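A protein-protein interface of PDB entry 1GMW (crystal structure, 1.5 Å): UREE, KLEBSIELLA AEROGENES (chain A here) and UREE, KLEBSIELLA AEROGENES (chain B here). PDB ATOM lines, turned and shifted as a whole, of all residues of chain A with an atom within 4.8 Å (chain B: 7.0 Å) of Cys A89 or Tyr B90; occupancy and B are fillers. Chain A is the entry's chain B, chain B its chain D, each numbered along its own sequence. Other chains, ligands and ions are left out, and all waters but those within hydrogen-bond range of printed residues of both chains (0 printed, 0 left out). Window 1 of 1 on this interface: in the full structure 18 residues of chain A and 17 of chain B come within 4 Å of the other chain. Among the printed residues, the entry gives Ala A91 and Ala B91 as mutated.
Among the printed residues, merely in contact across the chains: Ala A86 with Cys B89 (3.6 Å), Cys A89 with Ala B86 (3.6 Å), Cys A89 with Tyr B90 (3.5 Å), Tyr A90 with Cys B89 (3.6 Å), Tyr A90 with Gly B93 (3.6 Å), Tyr A90 with Ile B101 (3.7 Å), Gly A93 with Tyr B90 (3.6 Å), Gly A93 with Gly B93 (3.5 Å), Gly A93 with Asn B94 (3.5 Å), Pro A98 with Tyr B90 (3.6 Å), Ile A101 with Tyr B90 (3.7 Å), Glu A135 with Lys B87 (3.5 Å) and Ala A138 with Tyr B90 (3.8 Å).
SG of Cys A89 lies within hydrogen-bond range of O of Leu A85. O of Leu A92 lies within hydrogen-bond range of N of Val A97 (3.0 Å). The backbone carbonyl oxygen (O) of Leu A99 is in hydrogen-bond range of the backbone NH (N) of Glu A135 (2.9 Å). The side-chain sulfur (SG) of Cys B89 is in hydrogen-bond range of the backbone carbonyl oxygen (O) of Leu B85, at 3.2 Å. The backbone carbonyl oxygen (O) of Tyr B90 sits close to the side-chain amide oxygen (OD1) of Asn B94 (3.0 Å).
Cys A89 touches just these residues of chain B: Ala B86 and Tyr B90. Tyr B90 touches seven residues of chain A. Of the printed residues of chain A, Cys B89 touches Ala A86 and Tyr A90. Of the printed residues of chain B, Leu A99 touches Tyr B90. Printed residues of chain B within 4 Å of Val A97: Tyr B90. Ala B88 touches none of the printed residues of chain A. Leu A106 touches none of the printed residues of chain B. The nearest residue of chain B that does not touch Cys A89 is Cys B89 (4.4 Å). The nearest residue of chain A that does not touch Tyr B90 is Glu A135 (4.1 Å).
The backbone NH (N) of Leu B99 lies within hydrogen-bond range of the side-chain hydroxyl (OH) of Tyr A90 (3.5 Å). The side-chain hydroxyl (OH) of Tyr B90 sits at hydrogen-bond distance from the backbone carbonyl oxygen (O) of Val A97, at 2.6 Å. N of Leu A99 lies within hydrogen-bond range of OH of Tyr B90, 3.4 Å away.
Of the 15 printed residues of chain B, 8 touch a printed residue of chain A. Hydrophobic or aromatic side chains of chain A that line the printed part of chain B: Ala A86, Tyr A90, Leu A99, Ile A101 and Ala A138. Among the printed residues, 16 pairs touch across the chains.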
ATOM      1  N   LEU A  85     -12.683  -8.880   9.851  1.00  0.00           N
ATOM      2  CA  LEU A  85     -11.245  -9.051   9.721  1.00  0.00           C
ATOM      3  C   LEU A  85     -10.624  -9.177  11.111  1.00  0.00           C
ATOM      4  O   LEU A  85      -9.700  -9.960  11.323  1.00  0.00           O
ATOM      5  CB  LEU A  85     -10.603  -7.878   8.957  1.00  0.00           C
ATOM      6  CG  LEU A  85     -10.647  -7.959   7.424  1.00  0.00           C
ATOM      7  CD1 LEU A  85      -9.607  -7.023   6.833  1.00  0.00           C
ATOM      8  CD2 LEU A  85     -10.365  -9.389   6.960  1.00  0.00           C
ATOM      9  N   ALA A  86     -11.145  -8.404  12.055  1.00  0.00           N
ATOM     10  CA  ALA A  86     -10.649  -8.444  13.422  1.00  0.00           C
ATOM     11  C   ALA A  86     -10.840  -9.840  14.020  1.00  0.00           C
ATOM     12  O   ALA A  86      -9.979 -10.325  14.758  1.00  0.00           O
ATOM     13  CB  ALA A  86     -11.364  -7.401  14.274  1.00  0.00           C
ATOM     14  N   LYS A  87     -11.962 -10.484  13.698  1.00  0.00           N
ATOM     15  CA  LYS A  87     -12.225 -11.831  14.210  1.00  0.00           C
ATOM     16  C   LYS A  87     -11.248 -12.840  13.612  1.00  0.00           C
ATOM     17  O   LYS A  87     -10.878 -13.825  14.261  1.00  0.00           O
ATOM     18  CB  LYS A  87     -13.666 -12.266  13.903  1.00  0.00           C
ATOM     19  CG  LYS A  87     -14.726 -11.495  14.676  1.00  0.00           C
ATOM     20  CD  LYS A  87     -16.145 -11.964  14.348  1.00  0.00           C
ATOM     21  CE  LYS A  87     -16.460 -13.346  14.950  1.00  0.00           C
ATOM     22  NZ  LYS A  87     -15.731 -14.485  14.310  1.00  0.00           N
ATOM     23  N   ALA A  88     -10.837 -12.594  12.369  1.00  0.00           N
ATOM     24  CA  ALA A  88      -9.889 -13.475  11.694  1.00  0.00           C
ATOM     25  C   ALA A  88      -8.505 -13.223  12.294  1.00  0.00           C
ATOM     26  O   ALA A  88      -7.747 -14.167  12.540  1.00  0.00           O
ATOM     27  CB  ALA A  88      -9.881 -13.199  10.185  1.00  0.00           C
ATOM     28  N   CYS A  89      -8.190 -11.945  12.527  1.00  0.00           N
ATOM     29  CA  CYS A  89      -6.914 -11.558  13.123  1.00  0.00           C
ATOM     30  C   CYS A  89      -6.752 -12.217  14.485  1.00  0.00           C
ATOM     31  O   CYS A  89      -5.688 -12.753  14.807  1.00  0.00           O
ATOM     32  CB  CYS A  89      -6.820 -10.031  13.279  1.00  0.00           C
ATOM     33  SG  CYS A  89      -6.455  -9.107  11.763  1.00  0.00           S
ATOM     34  N   TYR A  90      -7.815 -12.180  15.285  1.00  0.00           N
ATOM     35  CA  TYR A  90      -7.783 -12.785  16.615  1.00  0.00           C
ATOM     36  C   TYR A  90      -7.580 -14.305  16.507  1.00  0.00           C
ATOM     37  O   TYR A  90      -6.787 -14.892  17.245  1.00  0.00           O
ATOM     38  CB  TYR A  90      -9.089 -12.491  17.359  1.00  0.00           C
ATOM     39  CG  TYR A  90      -9.182 -13.175  18.700  1.00  0.00           C
ATOM     40  CD1 TYR A  90      -8.288 -12.863  19.726  1.00  0.00           C
ATOM     41  CD2 TYR A  90     -10.137 -14.165  18.937  1.00  0.00           C
ATOM     42  CE1 TYR A  90      -8.337 -13.520  20.958  1.00  0.00           C
ATOM     43  CE2 TYR A  90     -10.196 -14.833  20.168  1.00  0.00           C
ATOM     44  CZ  TYR A  90      -9.292 -14.505  21.173  1.00  0.00           C
ATOM     45  OH  TYR A  90      -9.330 -15.163  22.387  1.00  0.00           O
ATOM     46  N   ALA A  91      -8.291 -14.925  15.567  1.00  0.00           N
ATOM     47  CA  ALA A  91      -8.220 -16.364  15.364  1.00  0.00           C
ATOM     48  C   ALA A  91      -6.859 -16.801  14.850  1.00  0.00           C
ATOM     49  O   ALA A  91      -6.367 -17.869  15.209  1.00  0.00           O
ATOM     50  CB  ALA A  91      -9.327 -16.818  14.399  1.00  0.00           C
ATOM     51  N   LEU A  92      -6.247 -15.975  14.010  1.00  0.00           N
ATOM     52  CA  LEU A  92      -4.935 -16.312  13.471  1.00  0.00           C
ATOM     53  C   LEU A  92      -3.860 -16.059  14.518  1.00  0.00           C
ATOM     54  O   LEU A  92      -2.873 -16.785  14.579  1.00  0.00           O
ATOM     55  CB  LEU A  92      -4.673 -15.509  12.198  1.00  0.00           C
ATOM     56  CG  LEU A  92      -5.655 -15.899  11.087  1.00  0.00           C
ATOM     57  CD1 LEU A  92      -5.708 -14.845   9.996  1.00  0.00           C
ATOM     58  CD2 LEU A  92      -5.243 -17.222  10.538  1.00  0.00           C
ATOM     59  N   GLY A  93      -4.050 -15.035  15.347  1.00  0.00           N
ATOM     60  CA  GLY A  93      -3.082 -14.786  16.394  1.00  0.00           C
ATOM     61  C   GLY A  93      -3.102 -15.987  17.324  1.00  0.00           C
ATOM     62  O   GLY A  93      -2.055 -16.483  17.763  1.00  0.00           O
ATOM     63  N   VAL A  97      -0.109 -17.564  13.646  1.00  0.00           N
ATOM     64  CA  VAL A  97       0.138 -17.411  12.219  1.00  0.00           C
ATOM     65  C   VAL A  97       0.745 -16.035  11.924  1.00  0.00           C
ATOM     66  O   VAL A  97       0.130 -15.013  12.210  1.00  0.00           O
ATOM     67  CB  VAL A  97      -1.193 -17.539  11.418  1.00  0.00           C
ATOM     68  CG1 VAL A  97      -0.942 -17.352   9.937  1.00  0.00           C
ATOM     69  CG2 VAL A  97      -1.840 -18.893  11.681  1.00  0.00           C
ATOM     70  N   PRO A  98       1.966 -15.988  11.364  1.00  0.00           N
ATOM     71  CA  PRO A  98       2.552 -14.672  11.066  1.00  0.00           C
ATOM     72  C   PRO A  98       1.573 -14.012  10.105  1.00  0.00           C
ATOM     73  O   PRO A  98       1.198 -14.606   9.089  1.00  0.00           O
ATOM     74  CB  PRO A  98       3.883 -15.029  10.411  1.00  0.00           C
ATOM     75  CG  PRO A  98       4.232 -16.331  11.079  1.00  0.00           C
ATOM     76  CD  PRO A  98       2.919 -17.067  11.049  1.00  0.00           C
ATOM     77  N   LEU A  99       1.155 -12.792  10.421  1.00  0.00           N
ATOM     78  CA  LEU A  99       0.155 -12.122   9.612  1.00  0.00           C
ATOM     79  C   LEU A  99       0.453 -10.674   9.243  1.00  0.00           C
ATOM     80  O   LEU A  99       0.990  -9.892  10.044  1.00  0.00           O
ATOM     81  CB  LEU A  99      -1.196 -12.190  10.346  1.00  0.00           C
ATOM     82  CG  LEU A  99      -2.477 -11.668   9.674  1.00  0.00           C
ATOM     83  CD1 LEU A  99      -2.997 -12.688   8.680  1.00  0.00           C
ATOM     84  CD2 LEU A  99      -3.545 -11.411  10.734  1.00  0.00           C
ATOM     85  N   ILE A 101      -1.249  -7.267   8.347  1.00  0.00           N
ATOM     86  CA  ILE A 101      -2.530  -6.629   8.555  1.00  0.00           C
ATOM     87  C   ILE A 101      -2.588  -5.227   7.940  1.00  0.00           C
ATOM     88  O   ILE A 101      -1.793  -4.352   8.291  1.00  0.00           O
ATOM     89  CB  ILE A 101      -2.844  -6.532  10.067  1.00  0.00           C
ATOM     90  CG1 ILE A 101      -2.852  -7.931  10.686  1.00  0.00           C
ATOM     91  CG2 ILE A 101      -4.192  -5.845  10.275  1.00  0.00           C
ATOM     92  CD1 ILE A 101      -3.027  -7.931  12.193  1.00  0.00           C
ATOM     93  N   LEU A 106      -5.621  -8.995   4.642  1.00  0.00           N
ATOM     94  CA  LEU A 106      -4.709  -9.718   5.513  1.00  0.00           C
ATOM     95  C   LEU A 106      -3.932 -10.651   4.582  1.00  0.00           C
ATOM     96  O   LEU A 106      -4.438 -11.039   3.527  1.00  0.00           O
ATOM     97  CB  LEU A 106      -5.485 -10.544   6.556  1.00  0.00           C
ATOM     98  CG  LEU A 106      -6.642  -9.881   7.320  1.00  0.00           C
ATOM     99  CD1 LEU A 106      -7.183 -10.853   8.354  1.00  0.00           C
ATOM    100  CD2 LEU A 106      -6.179  -8.610   7.986  1.00  0.00           C
ATOM    101  N   GLU A 135       3.377  -8.562  11.071  1.00  0.00           N
ATOM    102  CA  GLU A 135       3.635  -7.818  12.308  1.00  0.00           C
ATOM    103  C   GLU A 135       4.812  -8.446  13.053  1.00  0.00           C
ATOM    104  O   GLU A 135       5.056  -9.642  12.935  1.00  0.00           O
ATOM    105  CB  GLU A 135       2.408  -7.854  13.225  1.00  0.00           C
ATOM    106  CG  GLU A 135       1.191  -7.106  12.711  1.00  0.00           C
ATOM    107  CD  GLU A 135       1.370  -5.599  12.731  1.00  0.00           C
ATOM    108  OE1 GLU A 135       1.997  -5.039  11.802  1.00  0.00           O
ATOM    109  OE2 GLU A 135       0.882  -4.971  13.692  1.00  0.00           O
ATOM    110  N   ALA A 138       5.478 -12.592  15.460  1.00  0.00           N
ATOM    111  CA  ALA A 138       5.452 -13.996  15.056  1.00  0.00           C
ATOM    112  C   ALA A 138       6.859 -14.507  14.747  1.00  0.00           C
ATOM    113  O   ALA A 138       7.151 -14.762  13.556  1.00  0.00           O
ATOM    114  CB  ALA A 138       4.548 -14.170  13.837  1.00  0.00           C
ATOM    115  OXT ALA A 138       7.657 -14.641  15.704  1.00  0.00           O
ATOM    116  N   MET B  84      -6.690  -0.212  13.886  1.00  0.00           N
ATOM    117  CA  MET B  84      -5.942  -0.390  15.126  1.00  0.00           C
ATOM    118  C   MET B  84      -6.511  -1.519  15.984  1.00  0.00           C
ATOM    119  O   MET B  84      -5.766  -2.195  16.694  1.00  0.00           O
ATOM    120  CB  MET B  84      -5.927   0.906  15.938  1.00  0.00           C
ATOM    121  CG  MET B  84      -5.093   2.024  15.332  1.00  0.00           C
ATOM    122  SD  MET B  84      -5.112   3.614  16.443  1.00  0.00           S
ATOM    123  CE  MET B  84      -3.731   3.105  17.712  1.00  0.00           C
ATOM    124  N   LEU B  85      -7.825  -1.722  15.930  1.00  0.00           N
ATOM    125  CA  LEU B  85      -8.437  -2.785  16.716  1.00  0.00           C
ATOM    126  C   LEU B  85      -7.989  -4.140  16.213  1.00  0.00           C
ATOM    127  O   LEU B  85      -7.709  -5.040  17.010  1.00  0.00           O
ATOM    128  CB  LEU B  85      -9.967  -2.713  16.670  1.00  0.00           C
ATOM    129  CG  LEU B  85     -10.654  -1.659  17.540  1.00  0.00           C
ATOM    130  CD1 LEU B  85     -12.130  -2.015  17.686  1.00  0.00           C
ATOM    131  CD2 LEU B  85      -9.999  -1.608  18.910  1.00  0.00           C
ATOM    132  N   ALA B  86      -7.918  -4.277  14.893  1.00  0.00           N
ATOM    133  CA  ALA B  86      -7.504  -5.533  14.274  1.00  0.00           C
ATOM    134  C   ALA B  86      -6.106  -5.919  14.766  1.00  0.00           C
ATOM    135  O   ALA B  86      -5.853  -7.081  15.093  1.00  0.00           O
ATOM    136  CB  ALA B  86      -7.525  -5.406  12.746  1.00  0.00           C
ATOM    137  N   LYS B  87      -5.211  -4.937  14.829  1.00  0.00           N
ATOM    138  CA  LYS B  87      -3.863  -5.180  15.314  1.00  0.00           C
ATOM    139  C   LYS B  87      -3.898  -5.567  16.796  1.00  0.00           C
ATOM    140  O   LYS B  87      -3.144  -6.434  17.240  1.00  0.00           O
ATOM    141  CB  LYS B  87      -2.987  -3.942  15.083  1.00  0.00           C
ATOM    142  CG  LYS B  87      -2.569  -3.788  13.624  1.00  0.00           C
ATOM    143  CD  LYS B  87      -1.634  -2.616  13.389  1.00  0.00           C
ATOM    144  CE  LYS B  87      -2.376  -1.291  13.406  1.00  0.00           C
ATOM    145  NZ  LYS B  87      -1.451  -0.145  13.179  1.00  0.00           N
ATOM    146  N   ALA B  88      -4.784  -4.937  17.560  1.00  0.00           N
ATOM    147  CA  ALA B  88      -4.903  -5.255  18.975  1.00  0.00           C
ATOM    148  C   ALA B  88      -5.403  -6.693  19.113  1.00  0.00           C
ATOM    149  O   ALA B  88      -4.895  -7.457  19.934  1.00  0.00           O
ATOM    150  CB  ALA B  88      -5.871  -4.281  19.663  1.00  0.00           C
ATOM    151  N   CYS B  89      -6.396  -7.062  18.310  1.00  0.00           N
ATOM    152  CA  CYS B  89      -6.926  -8.425  18.349  1.00  0.00           C
ATOM    153  C   CYS B  89      -5.824  -9.433  18.084  1.00  0.00           C
ATOM    154  O   CYS B  89      -5.774 -10.485  18.728  1.00  0.00           O
ATOM    155  CB  CYS B  89      -8.016  -8.629  17.296  1.00  0.00           C
ATOM    156  SG  CYS B  89      -9.481  -7.645  17.573  1.00  0.00           S
ATOM    157  N   TYR B  90      -4.941  -9.110  17.143  1.00  0.00           N
ATOM    158  CA  TYR B  90      -3.856 -10.016  16.788  1.00  0.00           C
ATOM    159  C   TYR B  90      -2.927 -10.267  17.963  1.00  0.00           C
ATOM    160  O   TYR B  90      -2.684 -11.420  18.329  1.00  0.00           O
ATOM    161  CB  TYR B  90      -3.048  -9.464  15.610  1.00  0.00           C
ATOM    162  CG  TYR B  90      -1.995 -10.431  15.119  1.00  0.00           C
ATOM    163  CD1 TYR B  90      -2.363 -11.654  14.550  1.00  0.00           C
ATOM    164  CD2 TYR B  90      -0.633 -10.140  15.250  1.00  0.00           C
ATOM    165  CE1 TYR B  90      -1.400 -12.566  14.122  1.00  0.00           C
ATOM    166  CE2 TYR B  90       0.344 -11.046  14.823  1.00  0.00           C
ATOM    167  CZ  TYR B  90      -0.048 -12.260  14.258  1.00  0.00           C
ATOM    168  OH  TYR B  90       0.895 -13.168  13.822  1.00  0.00           O
ATOM    169  N   ALA B  91      -2.412  -9.183  18.543  1.00  0.00           N
ATOM    170  CA  ALA B  91      -1.508  -9.266  19.686  1.00  0.00           C
ATOM    171  C   ALA B  91      -2.174 -10.028  20.822  1.00  0.00           C
ATOM    172  O   ALA B  91      -1.570 -10.927  21.411  1.00  0.00           O
ATOM    173  CB  ALA B  91      -1.104  -7.860  20.174  1.00  0.00           C
ATOM    174  N   LEU B  92      -3.408  -9.660  21.142  1.00  0.00           N
ATOM    175  CA  LEU B  92      -4.131 -10.332  22.215  1.00  0.00           C
ATOM    176  C   LEU B  92      -4.309 -11.800  21.843  1.00  0.00           C
ATOM    177  O   LEU B  92      -4.167 -12.677  22.686  1.00  0.00           O
ATOM    178  CB  LEU B  92      -5.490  -9.666  22.437  1.00  0.00           C
ATOM    179  CG  LEU B  92      -5.421  -8.258  23.050  1.00  0.00           C
ATOM    180  CD1 LEU B  92      -6.761  -7.541  22.838  1.00  0.00           C
ATOM    181  CD2 LEU B  92      -5.060  -8.353  24.539  1.00  0.00           C
ATOM    182  N   GLY B  93      -4.608 -12.051  20.571  1.00  0.00           N
ATOM    183  CA  GLY B  93      -4.777 -13.410  20.095  1.00  0.00           C
ATOM    184  C   GLY B  93      -3.530 -14.238  20.331  1.00  0.00           C
ATOM    185  O   GLY B  93      -3.624 -15.403  20.707  1.00  0.00           O
ATOM    186  N   ASN B  94      -2.361 -13.634  20.113  1.00  0.00           N
ATOM    187  CA  ASN B  94      -1.073 -14.302  20.314  1.00  0.00           C
ATOM    188  C   ASN B  94      -0.812 -14.660  21.770  1.00  0.00           C
ATOM    189  O   ASN B  94      -0.047 -15.585  22.074  1.00  0.00           O
ATOM    190  CB  ASN B  94       0.074 -13.417  19.835  1.00  0.00           C
ATOM    191  CG  ASN B  94       0.368 -13.602  18.380  1.00  0.00           C
ATOM    192  OD1 ASN B  94      -0.152 -12.872  17.528  1.00  0.00           O
ATOM    193  ND2 ASN B  94       1.185 -14.610  18.069  1.00  0.00           N
ATOM    194  N   ARG B  95      -1.436 -13.911  22.668  1.00  0.00           N
ATOM    195  CA  ARG B  95      -1.272 -14.145  24.089  1.00  0.00           C
ATOM    196  C   ARG B  95      -2.379 -15.053  24.623  1.00  0.00           C
ATOM    197  O   ARG B  95      -2.463 -15.284  25.824  1.00  0.00           O
ATOM    198  CB  ARG B  95      -1.257 -12.806  24.832  1.00  0.00           C
ATOM    199  CG  ARG B  95      -0.371 -11.758  24.161  1.00  0.00           C
ATOM    200  CD  ARG B  95       0.562 -11.086  25.152  1.00  0.00           C
ATOM    201  NE  ARG B  95       1.449 -12.050  25.800  1.00  0.00           N
ATOM    202  CZ  ARG B  95       2.477 -11.720  26.575  1.00  0.00           C
ATOM    203  NH1 ARG B  95       2.762 -10.438  26.803  1.00  0.00           N
ATOM    204  NH2 ARG B  95       3.212 -12.672  27.139  1.00  0.00           N
ATOM    205  N   HIS B  96      -3.218 -15.563  23.721  1.00  0.00           N
ATOM    206  CA  HIS B  96      -4.318 -16.468  24.081  1.00  0.00           C
ATOM    207  C   HIS B  96      -5.247 -15.879  25.139  1.00  0.00           C
ATOM    208  O   HIS B  96      -5.707 -16.586  26.028  1.00  0.00           O
ATOM    209  CB  HIS B  96      -3.774 -17.807  24.604  1.00  0.00           C
ATOM    210  CG  HIS B  96      -2.841 -18.499  23.656  1.00  0.00           C
ATOM    211  ND1 HIS B  96      -3.207 -18.857  22.374  1.00  0.00           N
ATOM    212  CD2 HIS B  96      -1.561 -18.918  23.813  1.00  0.00           C
ATOM    213  CE1 HIS B  96      -2.194 -19.468  21.785  1.00  0.00           C
ATOM    214  NE2 HIS B  96      -1.184 -19.520  22.637  1.00  0.00           N
ATOM    215  N   LEU B  99     -11.255 -13.171  24.497  1.00  0.00           N
ATOM    216  CA  LEU B  99     -11.655 -11.857  24.077  1.00  0.00           C
ATOM    217  C   LEU B  99     -13.030 -11.744  23.444  1.00  0.00           C
ATOM    218  O   LEU B  99     -13.466 -12.610  22.669  1.00  0.00           O
ATOM    219  CB  LEU B  99     -10.592 -11.329  23.107  1.00  0.00           C
ATOM    220  CG  LEU B  99     -10.669  -9.894  22.585  1.00  0.00           C
ATOM    221  CD1 LEU B  99     -10.331  -8.951  23.719  1.00  0.00           C
ATOM    222  CD2 LEU B  99      -9.683  -9.701  21.430  1.00  0.00           C
ATOM    223  N   ILE B 101     -15.202  -9.502  20.979  1.00  0.00           N
ATOM    224  CA  ILE B 101     -14.926  -8.560  19.909  1.00  0.00           C
ATOM    225  C   ILE B 101     -16.203  -7.957  19.357  1.00  0.00           C
ATOM    226  O   ILE B 101     -17.156  -8.672  19.061  1.00  0.00           O
ATOM    227  CB  ILE B 101     -14.186  -9.257  18.751  1.00  0.00           C
ATOM    228  CG1 ILE B 101     -13.036 -10.099  19.305  1.00  0.00           C
ATOM    229  CG2 ILE B 101     -13.693  -8.223  17.745  1.00  0.00           C
ATOM    230  CD1 ILE B 101     -12.175 -10.734  18.240  1.00  0.00           C
